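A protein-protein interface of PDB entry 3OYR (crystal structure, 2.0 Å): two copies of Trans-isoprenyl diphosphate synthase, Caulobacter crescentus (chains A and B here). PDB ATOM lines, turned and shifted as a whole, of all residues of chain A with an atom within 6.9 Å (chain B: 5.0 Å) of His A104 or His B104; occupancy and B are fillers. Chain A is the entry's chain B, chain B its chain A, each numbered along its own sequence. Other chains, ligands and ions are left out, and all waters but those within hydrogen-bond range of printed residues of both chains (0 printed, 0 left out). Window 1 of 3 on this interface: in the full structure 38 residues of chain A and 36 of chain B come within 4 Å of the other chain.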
ATOM      1  N   THR A  99      15.153 -18.194  -4.775  1.00  0.00           N
ATOM      2  CA  THR A  99      13.830 -17.666  -5.112  1.00  0.00           C
ATOM      3  C   THR A  99      13.288 -16.778  -4.019  1.00  0.00           C
ATOM      4  O   THR A  99      12.760 -15.705  -4.291  1.00  0.00           O
ATOM      5  CB  THR A  99      12.801 -18.808  -5.423  1.00  0.00           C
ATOM      6  OG1 THR A  99      13.333 -19.669  -6.442  1.00  0.00           O
ATOM      7  CG2 THR A  99      11.484 -18.212  -5.899  1.00  0.00           C
ATOM      8  N   ALA A 100      13.427 -17.237  -2.779  1.00  0.00           N
ATOM      9  CA  ALA A 100      13.023 -16.458  -1.617  1.00  0.00           C
ATOM     10  C   ALA A 100      13.771 -15.128  -1.491  1.00  0.00           C
ATOM     11  O   ALA A 100      13.165 -14.097  -1.138  1.00  0.00           O
ATOM     12  CB  ALA A 100      13.227 -17.273  -0.363  1.00  0.00           C
ATOM     13  N   THR A 101      15.078 -15.149  -1.765  1.00  0.00           N
ATOM     14  CA  THR A 101      15.880 -13.926  -1.659  1.00  0.00           C
ATOM     15  C   THR A 101      15.469 -12.930  -2.737  1.00  0.00           C
ATOM     16  O   THR A 101      15.499 -11.735  -2.496  1.00  0.00           O
ATOM     17  CB  THR A 101      17.400 -14.158  -1.818  1.00  0.00           C
ATOM     18  OG1 THR A 101      17.678 -14.576  -3.157  1.00  0.00           O
ATOM     19  CG2 THR A 101      17.918 -15.182  -0.810  1.00  0.00           C
ATOM     20  N   LEU A 102      15.094 -13.435  -3.912  1.00  0.00           N
ATOM     21  CA  LEU A 102      14.510 -12.590  -4.969  1.00  0.00           C
ATOM     22  C   LEU A 102      13.243 -11.864  -4.541  1.00  0.00           C
ATOM     23  O   LEU A 102      13.118 -10.652  -4.757  1.00  0.00           O
ATOM     24  CB  LEU A 102      14.233 -13.388  -6.243  1.00  0.00           C
ATOM     25  CG  LEU A 102      15.439 -14.044  -6.909  1.00  0.00           C
ATOM     26  CD1 LEU A 102      14.992 -14.774  -8.160  1.00  0.00           C
ATOM     27  CD2 LEU A 102      16.562 -13.027  -7.236  1.00  0.00           C
ATOM     28  N   LEU A 103      12.313 -12.605  -3.937  1.00  0.00           N
ATOM     29  CA  LEU A 103      11.053 -12.023  -3.488  1.00  0.00           C
ATOM     30  C   LEU A 103      11.316 -10.920  -2.470  1.00  0.00           C
ATOM     31  O   LEU A 103      10.769  -9.833  -2.578  1.00  0.00           O
ATOM     32  CB  LEU A 103      10.128 -13.097  -2.912  1.00  0.00           C
ATOM     33  CG  LEU A 103       9.511 -14.069  -3.933  1.00  0.00           C
ATOM     34  CD1 LEU A 103       8.806 -15.204  -3.236  1.00  0.00           C
ATOM     35  CD2 LEU A 103       8.563 -13.374  -4.893  1.00  0.00           C
ATOM     36  N   HIS A 104      12.201 -11.201  -1.518  1.00  0.00           N
ATOM     37  CA  HIS A 104      12.549 -10.258  -0.484  1.00  0.00           C
ATOM     38  C   HIS A 104      13.339  -9.079  -1.046  1.00  0.00           C
ATOM     39  O   HIS A 104      13.044  -7.924  -0.711  1.00  0.00           O
ATOM     40  CB  HIS A 104      13.304 -10.973   0.641  1.00  0.00           C
ATOM     41  CG  HIS A 104      12.422 -11.837   1.488  1.00  0.00           C
ATOM     42  ND1 HIS A 104      12.756 -12.209   2.769  1.00  0.00           N
ATOM     43  CD2 HIS A 104      11.200 -12.376   1.245  1.00  0.00           C
ATOM     44  CE1 HIS A 104      11.778 -12.930   3.284  1.00  0.00           C
ATOM     45  NE2 HIS A 104      10.825 -13.050   2.379  1.00  0.00           N
ATOM     46  N   ASP A 105      14.294  -9.358  -1.931  1.00  0.00           N
ATOM     47  CA  ASP A 105      15.151  -8.304  -2.440  1.00  0.00           C
ATOM     48  C   ASP A 105      14.364  -7.360  -3.354  1.00  0.00           C
ATOM     49  O   ASP A 105      14.538  -6.148  -3.272  1.00  0.00           O
ATOM     50  CB  ASP A 105      16.370  -8.894  -3.142  1.00  0.00           C
ATOM     51  CG  ASP A 105      17.281  -7.831  -3.739  1.00  0.00           C
ATOM     52  OD1 ASP A 105      18.054  -7.189  -3.001  1.00  0.00           O
ATOM     53  OD2 ASP A 105      17.229  -7.638  -4.971  1.00  0.00           O
ATOM     54  N   ASP A 106      13.472  -7.906  -4.185  1.00  0.00           N
ATOM     55  CA  ASP A 106      12.594  -7.066  -5.020  1.00  0.00           C
ATOM     56  C   ASP A 106      11.660  -6.163  -4.224  1.00  0.00           C
ATOM     57  O   ASP A 106      11.390  -5.033  -4.655  1.00  0.00           O
ATOM     58  CB  ASP A 106      11.771  -7.902  -6.000  1.00  0.00           C
ATOM     59  CG  ASP A 106      12.577  -8.367  -7.201  1.00  0.00           C
ATOM     60  OD1 ASP A 106      13.561  -7.685  -7.593  1.00  0.00           O
ATOM     61  OD2 ASP A 106      12.222  -9.435  -7.747  1.00  0.00           O
ATOM     62  N   VAL A 107      11.174  -6.647  -3.076  1.00  0.00           N
ATOM     63  CA  VAL A 107      10.351  -5.830  -2.186  1.00  0.00           C
ATOM     64  C   VAL A 107      11.170  -4.692  -1.556  1.00  0.00           C
ATOM     65  O   VAL A 107      10.712  -3.552  -1.466  1.00  0.00           O
ATOM     66  CB  VAL A 107       9.677  -6.703  -1.086  1.00  0.00           C
ATOM     67  CG1 VAL A 107       9.103  -5.858   0.036  1.00  0.00           C
ATOM     68  CG2 VAL A 107       8.590  -7.540  -1.694  1.00  0.00           C
ATOM     69  N   VAL A 108      12.383  -5.024  -1.126  1.00  0.00           N
ATOM     70  CA  VAL A 108      13.288  -4.081  -0.479  1.00  0.00           C
ATOM     71  C   VAL A 108      13.735  -2.988  -1.466  1.00  0.00           C
ATOM     72  O   VAL A 108      13.653  -1.789  -1.170  1.00  0.00           O
ATOM     73  CB  VAL A 108      14.480  -4.847   0.152  1.00  0.00           C
ATOM     74  CG1 VAL A 108      15.657  -3.919   0.465  1.00  0.00           C
ATOM     75  CG2 VAL A 108      14.011  -5.563   1.413  1.00  0.00           C
ATOM     76  N   ASP A 109      14.155  -3.405  -2.654  1.00  0.00           N
ATOM     77  CA  ASP A 109      14.644  -2.472  -3.660  1.00  0.00           C
ATOM     78  C   ASP A 109      13.537  -1.690  -4.388  1.00  0.00           C
ATOM     79  O   ASP A 109      13.811  -0.671  -5.029  1.00  0.00           O
ATOM     80  CB  ASP A 109      15.483  -3.226  -4.678  1.00  0.00           C
ATOM     81  CG  ASP A 109      16.869  -3.521  -4.185  1.00  0.00           C
ATOM     82  OD1 ASP A 109      17.569  -4.321  -4.855  1.00  0.00           O
ATOM     83  OD2 ASP A 109      17.266  -2.971  -3.137  1.00  0.00           O
ATOM     84  N   GLY A 110      12.300  -2.168  -4.301  1.00  0.00           N
ATOM     85  CA  GLY A 110      11.185  -1.586  -5.053  1.00  0.00           C
ATOM     86  C   GLY A 110      11.205  -1.839  -6.560  1.00  0.00           C
ATOM     87  O   GLY A 110      10.671  -1.033  -7.324  1.00  0.00           O
ATOM     88  N   GLY A 126       3.338  -6.541  -0.889  1.00  0.00           N
ATOM     89  CA  GLY A 126       4.641  -6.711  -0.251  1.00  0.00           C
ATOM     90  C   GLY A 126       4.615  -7.765   0.837  1.00  0.00           C
ATOM     91  O   GLY A 126       5.509  -8.615   0.903  1.00  0.00           O
ATOM     92  N   ALA A 127       3.582  -7.733   1.672  1.00  0.00           N
ATOM     93  CA  ALA A 127       3.484  -8.653   2.805  1.00  0.00           C
ATOM     94  C   ALA A 127       3.468 -10.104   2.342  1.00  0.00           C
ATOM     95  O   ALA A 127       4.263 -10.923   2.842  1.00  0.00           O
ATOM     96  CB  ALA A 127       2.254  -8.338   3.656  1.00  0.00           C
ATOM     97  N   SER A 129       4.451 -11.347  -0.600  1.00  0.00           N
ATOM     98  CA  SER A 129       5.786 -11.630  -1.146  1.00  0.00           C
ATOM     99  C   SER A 129       6.792 -12.038  -0.083  1.00  0.00           C
ATOM    100  O   SER A 129       7.486 -13.062  -0.214  1.00  0.00           O
ATOM    101  CB  SER A 129       6.334 -10.416  -1.897  1.00  0.00           C
ATOM    102  OG  SER A 129       6.149 -10.576  -3.282  1.00  0.00           O
ATOM    103  N   VAL A 130       6.847 -11.255   0.980  1.00  0.00           N
ATOM    104  CA  VAL A 130       7.701 -11.579   2.124  1.00  0.00           C
ATOM    105  C   VAL A 130       7.356 -12.937   2.720  1.00  0.00           C
ATOM    106  O   VAL A 130       8.237 -13.782   2.867  1.00  0.00           O
ATOM    107  CB  VAL A 130       7.673 -10.446   3.170  1.00  0.00           C
ATOM    108  CG1 VAL A 130       8.217 -10.896   4.535  1.00  0.00           C
ATOM    109  CG2 VAL A 130       8.473  -9.286   2.631  1.00  0.00           C
ATOM    110  N   LEU A 131       6.073 -13.155   3.001  1.00  0.00           N
ATOM    111  CA  LEU A 131       5.595 -14.408   3.617  1.00  0.00           C
ATOM    112  C   LEU A 131       5.788 -15.672   2.770  1.00  0.00           C
ATOM    113  O   LEU A 131       6.143 -16.736   3.311  1.00  0.00           O
ATOM    114  CB  LEU A 131       4.143 -14.267   4.097  1.00  0.00           C
ATOM    115  CG  LEU A 131       3.817 -13.201   5.161  1.00  0.00           C
ATOM    116  CD1 LEU A 131       2.315 -13.155   5.444  1.00  0.00           C
ATOM    117  CD2 LEU A 131       4.603 -13.406   6.453  1.00  0.00           C
ATOM    118  N   VAL A 132       5.575 -15.564   1.462  1.00  0.00           N
ATOM    119  CA  VAL A 132       5.825 -16.682   0.539  1.00  0.00           C
ATOM    120  C   VAL A 132       7.323 -16.981   0.444  1.00  0.00           C
ATOM    121  O   VAL A 132       7.737 -18.151   0.417  1.00  0.00           O
ATOM    122  CB  VAL A 132       5.179 -16.465  -0.851  1.00  0.00           C
ATOM    123  CG1 VAL A 132       5.588 -17.578  -1.842  1.00  0.00           C
ATOM    124  CG2 VAL A 132       3.637 -16.430  -0.713  1.00  0.00           C
ATOM    125  N   GLY A 133       8.134 -15.928   0.462  1.00  0.00           N
ATOM    126  CA  GLY A 133       9.578 -16.101   0.632  1.00  0.00           C
ATOM    127  C   GLY A 133       9.901 -16.881   1.883  1.00  0.00           C
ATOM    128  O   GLY A 133      10.659 -17.856   1.808  1.00  0.00           O
ATOM    129  N   ASP A 134       9.307 -16.494   3.023  1.00  0.00           N
ATOM    130  CA  ASP A 134       9.469 -17.264   4.283  1.00  0.00           C
ATOM    131  C   ASP A 134       9.066 -18.737   4.158  1.00  0.00           C
ATOM    132  O   ASP A 134       9.766 -19.606   4.681  1.00  0.00           O
ATOM    133  CB  ASP A 134       8.728 -16.613   5.463  1.00  0.00           C
ATOM    134  CG  ASP A 134       9.250 -15.226   5.789  1.00  0.00           C
ATOM    135  OD1 ASP A 134      10.354 -14.871   5.304  1.00  0.00           O
ATOM    136  OD2 ASP A 134       8.553 -14.485   6.534  1.00  0.00           O
ATOM    137  N   PHE A 135       7.967 -19.008   3.443  1.00  0.00           N
ATOM    138  CA  PHE A 135       7.531 -20.384   3.102  1.00  0.00           C
ATOM    139  C   PHE A 135       8.607 -21.177   2.334  1.00  0.00           C
ATOM    140  O   PHE A 135       8.942 -22.325   2.695  1.00  0.00           O
ATOM    141  CB  PHE A 135       6.211 -20.356   2.291  1.00  0.00           C
ATOM    142  CG  PHE A 135       5.760 -21.732   1.779  1.00  0.00           C
ATOM    143  CD1 PHE A 135       5.015 -22.582   2.585  1.00  0.00           C
ATOM    144  CD2 PHE A 135       6.092 -22.159   0.484  1.00  0.00           C
ATOM    145  CE1 PHE A 135       4.608 -23.840   2.116  1.00  0.00           C
ATOM    146  CE2 PHE A 135       5.685 -23.405   0.006  1.00  0.00           C
ATOM    147  CZ  PHE A 135       4.939 -24.243   0.820  1.00  0.00           C
ATOM    148  N   PHE A 137      11.794 -20.517   2.050  1.00  0.00           N
ATOM    149  CA  PHE A 137      12.968 -20.667   2.891  1.00  0.00           C
ATOM    150  C   PHE A 137      12.786 -21.881   3.790  1.00  0.00           C
ATOM    151  O   PHE A 137      13.680 -22.736   3.876  1.00  0.00           O
ATOM    152  CB  PHE A 137      13.220 -19.399   3.709  1.00  0.00           C
ATOM    153  CG  PHE A 137      14.529 -19.408   4.441  1.00  0.00           C
ATOM    154  CD1 PHE A 137      14.572 -19.562   5.821  1.00  0.00           C
ATOM    155  CD2 PHE A 137      15.719 -19.284   3.746  1.00  0.00           C
ATOM    156  CE1 PHE A 137      15.772 -19.572   6.498  1.00  0.00           C
ATOM    157  CE2 PHE A 137      16.918 -19.295   4.411  1.00  0.00           C
ATOM    158  CZ  PHE A 137      16.951 -19.427   5.796  1.00  0.00           C
ATOM    159  N   GLU A 167      22.897  -8.072   2.643  1.00  0.00           N
ATOM    160  CA  GLU A 167      21.802  -7.198   2.230  1.00  0.00           C
ATOM    161  C   GLU A 167      21.602  -6.033   3.195  1.00  0.00           C
ATOM    162  O   GLU A 167      21.301  -4.906   2.777  1.00  0.00           O
ATOM    163  CB  GLU A 167      20.511  -8.001   2.129  1.00  0.00           C
ATOM    164  CG  GLU A 167      20.451  -8.989   0.933  1.00  0.00           C
ATOM    165  CD  GLU A 167      19.900  -8.340  -0.321  1.00  0.00           C
ATOM    166  OE1 GLU A 167      20.591  -7.477  -0.911  1.00  0.00           O
ATOM    167  OE2 GLU A 167      18.772  -8.702  -0.715  1.00  0.00           O
ATOM    168  N   ALA B 100      11.821 -13.368  14.333  1.00  0.00           N
ATOM    169  CA  ALA B 100      11.774 -13.260  12.875  1.00  0.00           C
ATOM    170  C   ALA B 100      10.362 -13.126  12.336  1.00  0.00           C
ATOM    171  O   ALA B 100      10.119 -12.302  11.421  1.00  0.00           O
ATOM    172  CB  ALA B 100      12.480 -14.431  12.213  1.00  0.00           C
ATOM    173  N   THR B 101       9.431 -13.914  12.889  1.00  0.00           N
ATOM    174  CA  THR B 101       8.035 -13.884  12.426  1.00  0.00           C
ATOM    175  C   THR B 101       7.388 -12.554  12.796  1.00  0.00           C
ATOM    176  O   THR B 101       6.638 -11.998  11.998  1.00  0.00           O
ATOM    177  CB  THR B 101       7.168 -15.021  13.000  1.00  0.00           C
ATOM    178  OG1 THR B 101       7.142 -14.911  14.423  1.00  0.00           O
ATOM    179  CG2 THR B 101       7.704 -16.370  12.627  1.00  0.00           C
ATOM    180  N   LEU B 102       7.689 -12.039  13.990  1.00  0.00           N
ATOM    181  CA  LEU B 102       7.213 -10.697  14.391  1.00  0.00           C
ATOM    182  C   LEU B 102       7.750  -9.602  13.481  1.00  0.00           C
ATOM    183  O   LEU B 102       7.011  -8.699  13.105  1.00  0.00           O
ATOM    184  CB  LEU B 102       7.618 -10.357  15.823  1.00  0.00           C
ATOM    185  CG  LEU B 102       7.018 -11.143  16.989  1.00  0.00           C
ATOM    186  CD1 LEU B 102       7.744 -10.774  18.288  1.00  0.00           C
ATOM    187  CD2 LEU B 102       5.519 -10.910  17.103  1.00  0.00           C
ATOM    188  N   LEU B 103       9.035  -9.676  13.140  1.00  0.00           N
ATOM    189  CA  LEU B 103       9.636  -8.705  12.227  1.00  0.00           C
ATOM    190  C   LEU B 103       8.982  -8.689  10.837  1.00  0.00           C
ATOM    191  O   LEU B 103       8.860  -7.639  10.215  1.00  0.00           O
ATOM    192  CB  LEU B 103      11.135  -8.938  12.106  1.00  0.00           C
ATOM    193  CG  LEU B 103      11.958  -8.446  13.291  1.00  0.00           C
ATOM    194  CD1 LEU B 103      13.343  -9.031  13.203  1.00  0.00           C
ATOM    195  CD2 LEU B 103      12.021  -6.917  13.319  1.00  0.00           C
ATOM    196  N   HIS B 104       8.542  -9.852  10.369  1.00  0.00           N
ATOM    197  CA  HIS B 104       7.906  -9.948   9.070  1.00  0.00           C
ATOM    198  C   HIS B 104       6.410  -9.649   9.087  1.00  0.00           C
ATOM    199  O   HIS B 104       5.772  -9.671   8.039  1.00  0.00           O
ATOM    200  CB  HIS B 104       8.201 -11.311   8.452  1.00  0.00           C
ATOM    201  CG  HIS B 104       9.591 -11.431   7.909  1.00  0.00           C
ATOM    202  ND1 HIS B 104      10.019 -12.529   7.200  1.00  0.00           N
ATOM    203  CD2 HIS B 104      10.644 -10.579   7.950  1.00  0.00           C
ATOM    204  CE1 HIS B 104      11.274 -12.351   6.825  1.00  0.00           C
ATOM    205  NE2 HIS B 104      11.680 -11.179   7.276  1.00  0.00           N
ATOM    206  N   ASP B 105       5.863  -9.346  10.266  1.00  0.00           N
ATOM    207  CA  ASP B 105       4.440  -9.006  10.402  1.00  0.00           C
ATOM    208  C   ASP B 105       4.124  -7.518  10.258  1.00  0.00           C
ATOM    209  O   ASP B 105       3.098  -7.139   9.683  1.00  0.00           O
ATOM    210  CB  ASP B 105       3.863  -9.540  11.721  1.00  0.00           C
ATOM    211  CG  ASP B 105       3.199 -10.896  11.561  1.00  0.00           C
ATOM    212  OD1 ASP B 105       3.303 -11.498  10.467  1.00  0.00           O
ATOM    213  OD2 ASP B 105       2.560 -11.358  12.529  1.00  0.00           O
ATOM    214  N   ASP B 106       5.018  -6.674  10.753  1.00  0.00           N
ATOM    215  CA  ASP B 106       4.770  -5.230  10.808  1.00  0.00           C
ATOM    216  C   ASP B 106       5.015  -4.509   9.467  1.00  0.00           C
ATOM    217  O   ASP B 106       5.058  -3.279   9.418  1.00  0.00           O
ATOM    218  CB  ASP B 106       5.638  -4.600  11.915  1.00  0.00           C
ATOM    219  CG  ASP B 106       5.676  -5.436  13.204  1.00  0.00           C
ATOM    220  OD1 ASP B 106       4.679  -6.132  13.517  1.00  0.00           O
ATOM    221  OD2 ASP B 106       6.711  -5.386  13.910  1.00  0.00           O
ATOM    222  N   VAL B 107       5.133  -5.280   8.386  1.00  0.00           N
ATOM    223  CA  VAL B 107       5.804  -4.851   7.146  1.00  0.00           C
ATOM    224  C   VAL B 107       4.978  -3.957   6.191  1.00  0.00           C
ATOM    225  O   VAL B 107       5.545  -3.076   5.525  1.00  0.00           O
ATOM    226  CB  VAL B 107       6.493  -6.094   6.462  1.00  0.00           C
ATOM    227  CG1 VAL B 107       6.303  -6.155   4.943  1.00  0.00           C
ATOM    228  CG2 VAL B 107       7.945  -6.168   6.860  1.00  0.00           C
ATOM    229  N   SER B 129      13.486  -4.545   8.785  1.00  0.00           N
ATOM    230  CA  SER B 129      12.687  -5.606   9.388  1.00  0.00           C
ATOM    231  C   SER B 129      12.631  -6.895   8.556  1.00  0.00           C
ATOM    232  O   SER B 129      12.752  -7.995   9.105  1.00  0.00           O
ATOM    233  CB  SER B 129      11.266  -5.114   9.625  1.00  0.00           C
ATOM    234  OG  SER B 129      11.233  -4.268  10.737  1.00  0.00           O
ATOM    235  N   VAL B 130      12.467  -6.762   7.243  1.00  0.00           N
ATOM    236  CA  VAL B 130      12.529  -7.925   6.354  1.00  0.00           C
ATOM    237  C   VAL B 130      13.881  -8.651   6.497  1.00  0.00           C
ATOM    238  O   VAL B 130      13.942  -9.857   6.760  1.00  0.00           O
ATOM    239  CB  VAL B 130      12.269  -7.520   4.887  1.00  0.00           C
ATOM    240  CG1 VAL B 130      12.515  -8.705   3.911  1.00  0.00           C
ATOM    241  CG2 VAL B 130      10.856  -6.956   4.736  1.00  0.00           C
ATOM    242  N   LEU B 131      14.961  -7.896   6.378  1.00  0.00           N
ATOM    243  CA  LEU B 131      16.282  -8.498   6.302  1.00  0.00           C
ATOM    244  C   LEU B 131      16.828  -8.988   7.645  1.00  0.00           C
ATOM    245  O   LEU B 131      17.510 -10.012   7.697  1.00  0.00           O
ATOM    246  CB  LEU B 131      17.247  -7.527   5.613  1.00  0.00           C
ATOM    247  CG  LEU B 131      16.787  -7.073   4.223  1.00  0.00           C
ATOM    248  CD1 LEU B 131      17.553  -5.854   3.791  1.00  0.00           C
ATOM    249  CD2 LEU B 131      16.919  -8.214   3.212  1.00  0.00           C
ATOM    250  N   GLY B 133      14.839  -9.999  10.011  1.00  0.00           N
ATOM    251  CA  GLY B 133      14.038 -11.227  10.048  1.00  0.00           C
ATOM    252  C   GLY B 133      14.729 -12.388   9.346  1.00  0.00           C
ATOM    253  O   GLY B 133      14.898 -13.459   9.945  1.00  0.00           O
ATOM    254  N   ASP B 134      15.155 -12.180   8.100  1.00  0.00           N
ATOM    255  CA  ASP B 134      15.909 -13.218   7.364  1.00  0.00           C
ATOM    256  C   ASP B 134      17.189 -13.697   8.067  1.00  0.00           C
ATOM    257  O   ASP B 134      17.483 -14.905   8.116  1.00  0.00           O
ATOM    258  CB  ASP B 134      16.250 -12.728   5.958  1.00  0.00           C
ATOM    259  CG  ASP B 134      15.031 -12.571   5.096  1.00  0.00           C
ATOM    260  OD1 ASP B 134      13.936 -12.986   5.534  1.00  0.00           O
ATOM    261  OD2 ASP B 134      15.162 -12.043   3.971  1.00  0.00           O
ATOM    262  N   PHE B 137      16.077 -15.882  11.235  1.00  0.00           N
ATOM    263  CA  PHE B 137      15.555 -17.156  10.725  1.00  0.00           C
ATOM    264  C   PHE B 137      16.741 -18.075  10.429  1.00  0.00           C
ATOM    265  O   PHE B 137      16.780 -19.227  10.858  1.00  0.00           O
ATOM    266  CB  PHE B 137      14.737 -16.939   9.430  1.00  0.00           C
ATOM    267  CG  PHE B 137      13.233 -16.822   9.634  1.00  0.00           C
ATOM    268  CD1 PHE B 137      12.536 -17.729  10.426  1.00  0.00           C
ATOM    269  CD2 PHE B 137      12.508 -15.830   8.981  1.00  0.00           C
ATOM    270  CE1 PHE B 137      11.157 -17.610  10.586  1.00  0.00           C
ATOM    271  CE2 PHE B 137      11.118 -15.712   9.141  1.00  0.00           C
ATOM    272  CZ  PHE B 137      10.453 -16.593   9.937  1.00  0.00           C
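The side-chain carboxylate (OD2) of Asp B134 lies within hydrogen-bond range of a ring nitrogen (ND1) of His A104 (2.7 Å).
A ring nitrogen (ND1) of His B104 sits at hydrogen-bond distance from the side-chain carboxylate (OD2) of Asp A134 (2.5 Å).
His A104 touches three residues of chain B.
Of the printed residues of chain B, Val A130 touches His B104 (3.6 Å) and Val B130 (3.9 Å).
Printed residues of chain B within 4 Å of Asp A134: His B104 and Phe B137.
Of chain A, only His A104 (3.6 Å), Val A130 (3.6 Å) and Asp A134 (2.5 Å) come within 4 Å of His B104.
Of the printed residues of chain A, Asp B134 touches His A104 (2.7 Å).
Of the printed residues of chain A, Phe B137 touches Asp A134.
The nearest printed residue of chain B that does not touch His A104 is Leu B131 (5.2 Å).
The nearest residue of chain A that does not touch His B104 is Leu A131 (4.2 Å).
His A104 touches His B104 (CE1 to CE1, 3.6 Å).
His A104 touches Val B130 (ND1 to CG1, 3.7 Å).
His B104 touches Val A130.
Val A130 touches Val B130.
Phe B137 touches Asp A134.
Glu A167 touches Leu B131 (CB to CD2, 3.8 Å).
OD1 of Asp B134 sits close to NE2 of His B104 (3.4 Å).
The backbone carbonyl oxygen (O) of Val B130 lies within hydrogen-bond range of a ring nitrogen (NE2) of His B104 (2.7 Å).
The side-chain carboxylate of Asp A134 lies close to a ring nitrogen (NE2) of His A104, 3.5 Å away.
The backbone carbonyl oxygen of Val A130 lies within hydrogen-bond range of a ring nitrogen (NE2) of His A104, 2.7 Å away.
His A104 touches its own counterpart, His B104.
His A104 touches Val B130, and with the chains exchanged Val A130 touches His B104.
Val A130 touches its own counterpart, Val B130.
Asp A134 touches Phe B137, but with the chains exchanged Phe A137 does not touch Asp B134 (5.1 Å).
Positions printed for both chains: 100, 101, 102, 103, 104, 105, 106, 107, 129, 130, 131, 133, 134 and 137.
Of the 8 pairs that touch across the chains among the printed residues, 6 have their exchanged pair printed and touching as well.
Of the 23 printed residues of chain A, 4 touch a printed residue of chain B.
Of the 14 printed residues of chain B, 5 touch a printed residue of chain A.
Hydrophobic or aromatic side chains of chain B within 4 Å of the printed part of chain A: His B104, Val B130, Leu B131 and Phe B137.
Among the printed residues, 8 pairs touch across the chains.
Among the printed residues, no Asp or Glu carboxylate lies within 4 Å of a Lys or Arg side-chain nitrogen of the other chain.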
